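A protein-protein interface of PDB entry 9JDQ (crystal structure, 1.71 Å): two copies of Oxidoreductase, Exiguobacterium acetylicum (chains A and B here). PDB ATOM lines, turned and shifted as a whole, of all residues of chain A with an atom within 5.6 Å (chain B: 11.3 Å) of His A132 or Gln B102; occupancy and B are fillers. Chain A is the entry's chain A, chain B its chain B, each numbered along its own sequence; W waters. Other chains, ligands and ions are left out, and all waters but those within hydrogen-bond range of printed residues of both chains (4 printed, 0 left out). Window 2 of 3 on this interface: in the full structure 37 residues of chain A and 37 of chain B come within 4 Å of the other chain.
N of Leu B100 sits at hydrogen-bond distance from OD1 of Asn B153 (3.4 Å).
The backbone NH of Lys A181 sits at hydrogen-bond distance from the backbone carbonyl oxygen of His A132 (2.9 Å).
The backbone carbonyl oxygen (O) of His A132 is in hydrogen-bond range of the backbone NH (N) of Leu A182 (3.0 Å).
CG1 of Val B101 touches OG of Ser A125, at 3.8 Å.
OG of Ser A125 touches CD1 of Ile B104, at 3.5 Å.
Ala A128 touches Gln B102.
Arg A129 touches Gln B102 (CA to O, 3.6 Å).
CD of Glu A174 touches CD2 of Leu B100, 3.5 Å away.
Val B155 touches Glu A174 (CG2 to OE2, 3.5 Å).
His A132 touches one residue of chain B.
Of chain A, only Ala A128, Arg A129 and His A132 come within 4 Å of Gln B102.
Of chain B, only Val B101 (3.8 Å) and Ile B104 (3.5 Å) come within 4 Å of Ser A125.
No residue of chain B comes within 4 Å of Asp A133.
Ile A134 touches none of the printed residues of chain B.
No residue of chain B comes within 4 Å of Leu A175.
No residue of chain B comes within 4 Å of Ala A180.
Of the printed residues of chain A, Leu B100 touches Glu A174 (3.5 Å).
Of the printed residues of chain A, Ile B104 touches Ser A125 and Arg A129.
Of the printed residues of chain A, Val B155 touches Glu A174 (3.5 Å).
Of the printed residues of chain A, Val B101 touches Ser A125 (3.8 Å) and Glu A174 (2.8 Å).
The nearest printed residue of chain A that does not touch Val B101 is Ala A128 (4.1 Å).
Water W3 lies within hydrogen-bond range of the side-chain carboxylate (OE2) of Glu A174 (2.6 Å) and the backbone NH (N) of Asn B153 (2.8 Å).
Water W2 lies within hydrogen-bond range of the side-chain carboxylate (OE2) of Glu A174 (2.7 Å), the backbone carbonyl oxygen (O) of Asp B99 (2.7 Å) and the backbone NH (N) of Val B155 (3.1 Å).
Water W4 lies within hydrogen-bond range of the side-chain hydroxyl of Ser A125 and the side-chain hydroxyl of Thr B156.
Water W1 lies within hydrogen-bond range of OE1 of Gln B102, OE1 of Glu A174 and N of Val B101.
ND1 of His A132 is in hydrogen-bond range of NE2 of Gln B102, at 3.4 Å.
NH2 of Arg A129 is in hydrogen-bond range of O of Ile B104, 3.3 Å away.
The side-chain carboxylate (OE1) of Glu A174 sits at hydrogen-bond distance from the backbone NH (N) of Val B101 (2.8 Å).
No position is printed for both chains.
Of the 9 pairs that touch across the chains among the printed residues, none has its exchanged pair printed and touching as well.
Of the 15 printed residues of chain B, 5 touch a printed residue of chain A.
Of the 15 printed residues of chain A, 5 touch a printed residue of chain B.
Hydrophobic or aromatic side chains of chain A that line the printed part of chain B: His A132.
Among the printed residues, 9 pairs touch across the chains.
Among the printed residues, no Asp or Glu carboxylate lies within 4 Å of a Lys or Arg side-chain nitrogen of the other chain.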
ATOM      1  N   SER A 125      19.968   8.718  -2.337  1.00  0.00           N
ATOM      2  CA  SER A 125      19.848   7.282  -2.080  1.00  0.00           C
ATOM      3  C   SER A 125      18.528   6.777  -2.675  1.00  0.00           C
ATOM      4  O   SER A 125      18.476   5.750  -3.404  1.00  0.00           O
ATOM      5  CB  SER A 125      19.934   6.977  -0.612  1.00  0.00           C
ATOM      6  OG  SER A 125      21.234   7.232  -0.103  1.00  0.00           O
ATOM      7  N   PHE A 127      16.671   8.336  -4.955  1.00  0.00           N
ATOM      8  CA  PHE A 127      16.689   8.454  -6.402  1.00  0.00           C
ATOM      9  C   PHE A 127      17.438   7.255  -6.996  1.00  0.00           C
ATOM     10  O   PHE A 127      16.976   6.635  -7.953  1.00  0.00           O
ATOM     11  CB  PHE A 127      17.268   9.818  -6.776  1.00  0.00           C
ATOM     12  CG  PHE A 127      17.014  10.198  -8.216  1.00  0.00           C
ATOM     13  CD1 PHE A 127      15.720  10.343  -8.684  1.00  0.00           C
ATOM     14  CD2 PHE A 127      18.075  10.500  -9.064  1.00  0.00           C
ATOM     15  CE1 PHE A 127      15.486  10.707  -9.990  1.00  0.00           C
ATOM     16  CE2 PHE A 127      17.852  10.919 -10.353  1.00  0.00           C
ATOM     17  CZ  PHE A 127      16.551  10.994 -10.828  1.00  0.00           C
ATOM     18  N   ALA A 128      18.613   6.933  -6.444  1.00  0.00           N
ATOM     19  CA  ALA A 128      19.437   5.867  -6.994  1.00  0.00           C
ATOM     20  C   ALA A 128      18.707   4.528  -6.921  1.00  0.00           C
ATOM     21  O   ALA A 128      18.790   3.719  -7.843  1.00  0.00           O
ATOM     22  CB  ALA A 128      20.750   5.837  -6.273  1.00  0.00           C
ATOM     23  N   ARG A 129      17.975   4.308  -5.819  1.00  0.00           N
ATOM     24  CA  ARG A 129      17.286   3.057  -5.564  1.00  0.00           C
ATOM     25  C   ARG A 129      16.332   2.716  -6.713  1.00  0.00           C
ATOM     26  O   ARG A 129      16.197   1.539  -7.064  1.00  0.00           O
ATOM     27  CB  ARG A 129      16.529   3.211  -4.241  1.00  0.00           C
ATOM     28  CG  ARG A 129      15.608   2.081  -3.816  1.00  0.00           C
ATOM     29  CD  ARG A 129      14.880   2.277  -2.471  1.00  0.00           C
ATOM     30  NE  ARG A 129      15.738   2.257  -1.278  1.00  0.00           N
ATOM     31  CZ  ARG A 129      15.320   2.602  -0.052  1.00  0.00           C
ATOM     32  NH1 ARG A 129      14.070   2.982   0.152  1.00  0.00           N
ATOM     33  NH2 ARG A 129      16.167   2.619   0.958  1.00  0.00           N
ATOM     34  N   ASP A 130      15.622   3.717  -7.248  1.00  0.00           N
ATOM     35  CA  ASP A 130      14.609   3.412  -8.247  1.00  0.00           C
ATOM     36  C   ASP A 130      14.912   4.077  -9.599  1.00  0.00           C
ATOM     37  O   ASP A 130      14.080   3.956 -10.497  1.00  0.00           O
ATOM     38  CB  ASP A 130      13.199   3.591  -7.701  1.00  0.00           C
ATOM     39  CG  ASP A 130      12.820   5.001  -7.264  1.00  0.00           C
ATOM     40  OD1 ASP A 130      13.660   5.894  -7.419  1.00  0.00           O
ATOM     41  OD2 ASP A 130      11.703   5.190  -6.719  1.00  0.00           O
ATOM     42  N   HIS A 131      16.097   4.697  -9.791  1.00  0.00           N
ATOM     43  CA  HIS A 131      16.473   5.233 -11.091  1.00  0.00           C
ATOM     44  C   HIS A 131      17.770   4.635 -11.648  1.00  0.00           C
ATOM     45  O   HIS A 131      18.130   4.944 -12.774  1.00  0.00           O
ATOM     46  CB  HIS A 131      16.474   6.778 -11.103  1.00  0.00           C
ATOM     47  CG  HIS A 131      15.120   7.342 -10.873  1.00  0.00           C
ATOM     48  ND1 HIS A 131      14.536   7.390  -9.625  1.00  0.00           N
ATOM     49  CD2 HIS A 131      14.194   7.801 -11.740  1.00  0.00           C
ATOM     50  CE1 HIS A 131      13.301   7.859  -9.760  1.00  0.00           C
ATOM     51  NE2 HIS A 131      13.079   8.103 -11.041  1.00  0.00           N
ATOM     52  N   HIS A 132      18.507   3.809 -10.896  1.00  0.00           N
ATOM     53  CA  HIS A 132      19.855   3.427 -11.307  1.00  0.00           C
ATOM     54  C   HIS A 132      19.881   2.837 -12.727  1.00  0.00           C
ATOM     55  O   HIS A 132      20.829   3.086 -13.497  1.00  0.00           O
ATOM     56  CB  HIS A 132      20.491   2.441 -10.311  1.00  0.00           C
ATOM     57  CG  HIS A 132      19.724   1.167 -10.155  1.00  0.00           C
ATOM     58  ND1 HIS A 132      19.989   0.010 -10.872  1.00  0.00           N
ATOM     59  CD2 HIS A 132      18.650   0.899  -9.380  1.00  0.00           C
ATOM     60  CE1 HIS A 132      19.112  -0.921 -10.525  1.00  0.00           C
ATOM     61  NE2 HIS A 132      18.321  -0.428  -9.583  1.00  0.00           N
ATOM     62  N   ASP A 133      18.855   2.046 -13.069  1.00  0.00           N
ATOM     63  CA  ASP A 133      18.770   1.413 -14.391  1.00  0.00           C
ATOM     64  C   ASP A 133      17.795   2.113 -15.343  1.00  0.00           C
ATOM     65  O   ASP A 133      17.327   1.481 -16.302  1.00  0.00           O
ATOM     66  CB  ASP A 133      18.363  -0.053 -14.271  1.00  0.00           C
ATOM     67  CG  ASP A 133      17.073  -0.276 -13.495  1.00  0.00           C
ATOM     68  OD1 ASP A 133      16.549   0.723 -12.888  1.00  0.00           O
ATOM     69  OD2 ASP A 133      16.561  -1.425 -13.546  1.00  0.00           O
ATOM     70  N   ILE A 134      17.485   3.402 -15.124  1.00  0.00           N
ATOM     71  CA  ILE A 134      16.505   4.080 -15.971  1.00  0.00           C
ATOM     72  C   ILE A 134      17.216   5.059 -16.897  1.00  0.00           C
ATOM     73  O   ILE A 134      17.851   6.023 -16.449  1.00  0.00           O
ATOM     74  CB  ILE A 134      15.403   4.768 -15.137  1.00  0.00           C
ATOM     75  CG1 ILE A 134      14.598   3.760 -14.333  1.00  0.00           C
ATOM     76  CG2 ILE A 134      14.487   5.630 -16.020  1.00  0.00           C
ATOM     77  CD1 ILE A 134      13.493   4.374 -13.485  1.00  0.00           C
ATOM     78  N   THR A 137      18.407   9.452 -16.823  1.00  0.00           N
ATOM     79  CA  THR A 137      18.316  10.029 -15.477  1.00  0.00           C
ATOM     80  C   THR A 137      19.648  10.581 -14.980  1.00  0.00           C
ATOM     81  O   THR A 137      20.693   9.990 -15.213  1.00  0.00           O
ATOM     82  CB  THR A 137      17.762   8.972 -14.524  1.00  0.00           C
ATOM     83  OG1 THR A 137      18.594   7.809 -14.601  1.00  0.00           O
ATOM     84  CG2 THR A 137      16.338   8.605 -14.911  1.00  0.00           C
ATOM     85  N   GLU A 174      30.680   4.690  -8.793  1.00  0.00           N
ATOM     86  CA  GLU A 174      30.015   3.436  -8.513  1.00  0.00           C
ATOM     87  C   GLU A 174      29.057   3.132  -9.661  1.00  0.00           C
ATOM     88  O   GLU A 174      29.003   2.014 -10.176  1.00  0.00           O
ATOM     89  CB  GLU A 174      29.236   3.609  -7.205  1.00  0.00           C
ATOM     90  CG  GLU A 174      28.453   2.379  -6.786  1.00  0.00           C
ATOM     91  CD  GLU A 174      27.859   2.512  -5.396  1.00  0.00           C
ATOM     92  OE1 GLU A 174      26.655   2.778  -5.302  1.00  0.00           O
ATOM     93  OE2 GLU A 174      28.609   2.395  -4.410  1.00  0.00           O
ATOM     94  N   LEU A 175      28.309   4.155 -10.059  1.00  0.00           N
ATOM     95  CA  LEU A 175      27.329   3.952 -11.115  1.00  0.00           C
ATOM     96  C   LEU A 175      28.027   3.620 -12.445  1.00  0.00           C
ATOM     97  O   LEU A 175      27.642   2.672 -13.123  1.00  0.00           O
ATOM     98  CB  LEU A 175      26.429   5.179 -11.216  1.00  0.00           C
ATOM     99  CG  LEU A 175      25.473   5.407 -10.046  1.00  0.00           C
ATOM    100  CD1 LEU A 175      24.929   6.832 -10.136  1.00  0.00           C
ATOM    101  CD2 LEU A 175      24.355   4.399  -9.926  1.00  0.00           C
ATOM    102  N   ALA A 180      25.556   1.541 -14.753  1.00  0.00           N
ATOM    103  CA  ALA A 180      24.269   2.136 -14.459  1.00  0.00           C
ATOM    104  C   ALA A 180      23.848   3.045 -15.623  1.00  0.00           C
ATOM    105  O   ALA A 180      24.694   3.624 -16.299  1.00  0.00           O
ATOM    106  CB  ALA A 180      24.359   2.916 -13.169  1.00  0.00           C
ATOM    107  N   LYS A 181      22.541   3.235 -15.803  1.00  0.00           N
ATOM    108  CA  LYS A 181      22.055   4.246 -16.728  1.00  0.00           C
ATOM    109  C   LYS A 181      22.059   5.619 -16.063  1.00  0.00           C
ATOM    110  O   LYS A 181      22.328   6.627 -16.711  1.00  0.00           O
ATOM    111  CB  LYS A 181      20.623   3.993 -17.185  1.00  0.00           C
ATOM    112  CG  LYS A 181      20.374   2.672 -17.888  1.00  0.00           C
ATOM    113  CD  LYS A 181      21.232   2.417 -19.114  1.00  0.00           C
ATOM    114  CE  LYS A 181      20.822   1.140 -19.775  1.00  0.00           C
ATOM    115  NZ  LYS A 181      21.681   0.857 -20.925  1.00  0.00           N
ATOM    116  N   LEU A 182      21.741   5.654 -14.763  1.00  0.00           N
ATOM    117  CA  LEU A 182      21.815   6.886 -14.001  1.00  0.00           C
ATOM    118  C   LEU A 182      23.227   7.469 -13.984  1.00  0.00           C
ATOM    119  O   LEU A 182      24.211   6.763 -13.746  1.00  0.00           O
ATOM    120  CB  LEU A 182      21.335   6.583 -12.588  1.00  0.00           C
ATOM    121  CG  LEU A 182      21.422   7.736 -11.592  1.00  0.00           C
ATOM    122  CD1 LEU A 182      20.455   8.828 -11.947  1.00  0.00           C
ATOM    123  CD2 LEU A 182      21.215   7.212 -10.175  1.00  0.00           C
ATOM    124  N   ASP B  97      29.370   0.547   6.655  1.00  0.00           N
ATOM    125  CA  ASP B  97      28.397  -0.179   5.853  1.00  0.00           C
ATOM    126  C   ASP B  97      29.080  -0.566   4.549  1.00  0.00           C
ATOM    127  O   ASP B  97      29.928   0.198   4.070  1.00  0.00           O
ATOM    128  CB  ASP B  97      27.132   0.638   5.614  1.00  0.00           C
ATOM    129  CG  ASP B  97      25.999  -0.138   4.960  1.00  0.00           C
ATOM    130  OD1 ASP B  97      25.528  -1.143   5.586  1.00  0.00           O
ATOM    131  OD2 ASP B  97      25.598   0.249   3.866  1.00  0.00           O
ATOM    132  N   PHE B  98      28.712  -1.763   4.022  1.00  0.00           N
ATOM    133  CA  PHE B  98      29.109  -2.213   2.701  1.00  0.00           C
ATOM    134  C   PHE B  98      27.825  -2.482   1.930  1.00  0.00           C
ATOM    135  O   PHE B  98      26.992  -3.269   2.355  1.00  0.00           O
ATOM    136  CB  PHE B  98      29.997  -3.462   2.776  1.00  0.00           C
ATOM    137  CG  PHE B  98      31.237  -3.291   3.631  1.00  0.00           C
ATOM    138  CD1 PHE B  98      32.137  -2.265   3.383  1.00  0.00           C
ATOM    139  CD2 PHE B  98      31.475  -4.121   4.717  1.00  0.00           C
ATOM    140  CE1 PHE B  98      33.255  -2.089   4.182  1.00  0.00           C
ATOM    141  CE2 PHE B  98      32.603  -3.950   5.514  1.00  0.00           C
ATOM    142  CZ  PHE B  98      33.500  -2.948   5.232  1.00  0.00           C
ATOM    143  N   ASP B  99      27.669  -1.801   0.803  1.00  0.00           N
ATOM    144  CA  ASP B  99      26.530  -1.942  -0.083  1.00  0.00           C
ATOM    145  C   ASP B  99      26.611  -0.792  -1.062  1.00  0.00           C
ATOM    146  O   ASP B  99      27.151   0.258  -0.714  1.00  0.00           O
ATOM    147  CB  ASP B  99      25.163  -1.849   0.578  1.00  0.00           C
ATOM    148  CG  ASP B  99      24.470  -3.183   0.869  1.00  0.00           C
ATOM    149  OD1 ASP B  99      24.554  -4.103   0.041  1.00  0.00           O
ATOM    150  OD2 ASP B  99      23.791  -3.259   1.885  1.00  0.00           O
ATOM    151  N   LEU B 100      26.027  -1.001  -2.248  1.00  0.00           N
ATOM    152  CA  LEU B 100      25.915   0.067  -3.231  1.00  0.00           C
ATOM    153  C   LEU B 100      24.907   1.066  -2.689  1.00  0.00           C
ATOM    154  O   LEU B 100      24.023   0.688  -1.908  1.00  0.00           O
ATOM    155  CB  LEU B 100      25.443  -0.532  -4.557  1.00  0.00           C
ATOM    156  CG  LEU B 100      26.372  -1.539  -5.247  1.00  0.00           C
ATOM    157  CD1 LEU B 100      25.563  -2.156  -6.377  1.00  0.00           C
ATOM    158  CD2 LEU B 100      27.636  -0.917  -5.797  1.00  0.00           C
ATOM    159  N   VAL B 101      24.972   2.307  -3.175  1.00  0.00           N
ATOM    160  CA  VAL B 101      24.068   3.327  -2.674  1.00  0.00           C
ATOM    161  C   VAL B 101      22.618   2.902  -2.934  1.00  0.00           C
ATOM    162  O   VAL B 101      21.776   3.040  -2.066  1.00  0.00           O
ATOM    163  CB  VAL B 101      24.399   4.734  -3.220  1.00  0.00           C
ATOM    164  CG1 VAL B 101      23.278   5.754  -3.002  1.00  0.00           C
ATOM    165  CG2 VAL B 101      25.658   5.276  -2.575  1.00  0.00           C
ATOM    166  N   GLN B 102      22.325   2.418  -4.139  1.00  0.00           N
ATOM    167  CA  GLN B 102      20.965   2.038  -4.516  1.00  0.00           C
ATOM    168  C   GLN B 102      20.413   0.935  -3.607  1.00  0.00           C
ATOM    169  O   GLN B 102      19.200   0.705  -3.618  1.00  0.00           O
ATOM    170  CB  GLN B 102      20.974   1.593  -5.979  1.00  0.00           C
ATOM    171  CG  GLN B 102      21.695   0.261  -6.186  1.00  0.00           C
ATOM    172  CD  GLN B 102      22.152   0.029  -7.604  1.00  0.00           C
ATOM    173  OE1 GLN B 102      22.888   0.839  -8.171  1.00  0.00           O
ATOM    174  NE2 GLN B 102      21.778  -1.121  -8.156  1.00  0.00           N
ATOM    175  N   ASP B 103      21.300   0.259  -2.856  1.00  0.00           N
ATOM    176  CA  ASP B 103      20.951  -0.882  -2.022  1.00  0.00           C
ATOM    177  C   ASP B 103      20.901  -0.600  -0.512  1.00  0.00           C
ATOM    178  O   ASP B 103      20.561  -1.501   0.250  1.00  0.00           O
ATOM    179  CB  ASP B 103      21.923  -2.016  -2.289  1.00  0.00           C
ATOM    180  CG  ASP B 103      21.694  -2.785  -3.587  1.00  0.00           C
ATOM    181  OD1 ASP B 103      20.524  -2.766  -4.065  1.00  0.00           O
ATOM    182  OD2 ASP B 103      22.681  -3.396  -4.097  1.00  0.00           O
ATOM    183  N   ILE B 104      21.264   0.604  -0.049  1.00  0.00           N
ATOM    184  CA  ILE B 104      21.442   0.854   1.377  1.00  0.00           C
ATOM    185  C   ILE B 104      20.101   0.902   2.093  1.00  0.00           C
ATOM    186  O   ILE B 104      19.086   1.207   1.475  1.00  0.00           O
ATOM    187  CB  ILE B 104      22.245   2.141   1.662  1.00  0.00           C
ATOM    188  CG1 ILE B 104      21.664   3.395   0.981  1.00  0.00           C
ATOM    189  CG2 ILE B 104      23.709   1.911   1.342  1.00  0.00           C
ATOM    190  CD1 ILE B 104      21.040   4.378   1.948  1.00  0.00           C
ATOM    191  N   GLU B 105      20.141   0.566   3.392  1.00  0.00           N
ATOM    192  CA  GLU B 105      19.026   0.776   4.305  1.00  0.00           C
ATOM    193  C   GLU B 105      19.197   2.149   4.950  1.00  0.00           C
ATOM    194  O   GLU B 105      20.234   2.396   5.576  1.00  0.00           O
ATOM    195  CB  GLU B 105      19.003  -0.335   5.350  1.00  0.00           C
ATOM    196  CG  GLU B 105      17.663  -0.506   6.059  1.00  0.00           C
ATOM    197  CD  GLU B 105      17.457   0.429   7.236  1.00  0.00           C
ATOM    198  OE1 GLU B 105      18.285   0.452   8.169  1.00  0.00           O
ATOM    199  OE2 GLU B 105      16.441   1.126   7.221  1.00  0.00           O
ATOM    200  N   LEU B 106      18.196   3.027   4.759  1.00  0.00           N
ATOM    201  CA  LEU B 106      18.314   4.432   5.131  1.00  0.00           C
ATOM    202  C   LEU B 106      18.306   4.621   6.640  1.00  0.00           C
ATOM    203  O   LEU B 106      18.900   5.590   7.131  1.00  0.00           O
ATOM    204  CB  LEU B 106      17.301   5.336   4.415  1.00  0.00           C
ATOM    205  CG  LEU B 106      17.787   5.879   3.070  1.00  0.00           C
ATOM    206  CD1 LEU B 106      16.647   6.416   2.228  1.00  0.00           C
ATOM    207  CD2 LEU B 106      18.845   6.969   3.284  1.00  0.00           C
ATOM    208  N   ILE B 109      21.876   4.227   7.590  1.00  0.00           N
ATOM    209  CA  ILE B 109      22.764   5.244   7.024  1.00  0.00           C
ATOM    210  C   ILE B 109      22.473   6.573   7.714  1.00  0.00           C
ATOM    211  O   ILE B 109      23.378   7.306   8.138  1.00  0.00           O
ATOM    212  CB  ILE B 109      22.697   5.280   5.472  1.00  0.00           C
ATOM    213  CG1 ILE B 109      23.819   4.438   4.873  1.00  0.00           C
ATOM    214  CG2 ILE B 109      22.765   6.705   4.894  1.00  0.00           C
ATOM    215  CD1 ILE B 109      23.859   2.987   5.295  1.00  0.00           C
ATOM    216  N   ASN B 153      32.081   0.315  -2.739  1.00  0.00           N
ATOM    217  CA  ASN B 153      31.106  -0.438  -1.948  1.00  0.00           C
ATOM    218  C   ASN B 153      30.954   0.177  -0.551  1.00  0.00           C
ATOM    219  O   ASN B 153      30.192  -0.363   0.257  1.00  0.00           O
ATOM    220  CB  ASN B 153      31.388  -1.947  -1.943  1.00  0.00           C
ATOM    221  CG  ASN B 153      30.151  -2.809  -1.757  1.00  0.00           C
ATOM    222  OD1 ASN B 153      29.093  -2.556  -2.357  1.00  0.00           O
ATOM    223  ND2 ASN B 153      30.226  -3.823  -0.901  1.00  0.00           N
ATOM    224  N   ALA B 154      31.607   1.330  -0.296  1.00  0.00           N
ATOM    225  CA  ALA B 154      31.593   1.965   1.012  1.00  0.00           C
ATOM    226  C   ALA B 154      31.438   3.476   0.882  1.00  0.00           C
ATOM    227  O   ALA B 154      32.062   4.192   1.657  1.00  0.00           O
ATOM    228  CB  ALA B 154      32.870   1.625   1.757  1.00  0.00           C
ATOM    229  N   VAL B 155      30.669   3.930  -0.117  1.00  0.00           N
ATOM    230  CA  VAL B 155      30.684   5.342  -0.520  1.00  0.00           C
ATOM    231  C   VAL B 155      30.180   6.209   0.639  1.00  0.00           C
ATOM    232  O   VAL B 155      30.824   7.189   0.969  1.00  0.00           O
ATOM    233  CB  VAL B 155      29.902   5.573  -1.831  1.00  0.00           C
ATOM    234  CG1 VAL B 155      29.672   7.070  -2.166  1.00  0.00           C
ATOM    235  CG2 VAL B 155      30.641   4.895  -2.970  1.00  0.00           C
ATOM    236  N   THR B 156      29.067   5.825   1.281  1.00  0.00           N
ATOM    237  CA  THR B 156      28.459   6.679   2.292  1.00  0.00           C
ATOM    238  C   THR B 156      29.397   6.820   3.498  1.00  0.00           C
ATOM    239  O   THR B 156      29.664   7.924   3.973  1.00  0.00           O
ATOM    240  CB  THR B 156      27.084   6.178   2.717  1.00  0.00           C
ATOM    241  OG1 THR B 156      26.329   6.022   1.515  1.00  0.00           O
ATOM    242  CG2 THR B 156      26.425   7.211   3.600  1.00  0.00           C
HETATM  243  O   HOH W   1      24.027   2.740  -6.413  1.00  0.00           O
HETATM  244  O   HOH W   2      28.455   2.454  -1.711  1.00  0.00           O
HETATM  245  O   HOH W   3      31.092   1.653  -4.963  1.00  0.00           O
HETATM  246  O   HOH W   4      23.870   6.819   0.411  1.00  0.00           O
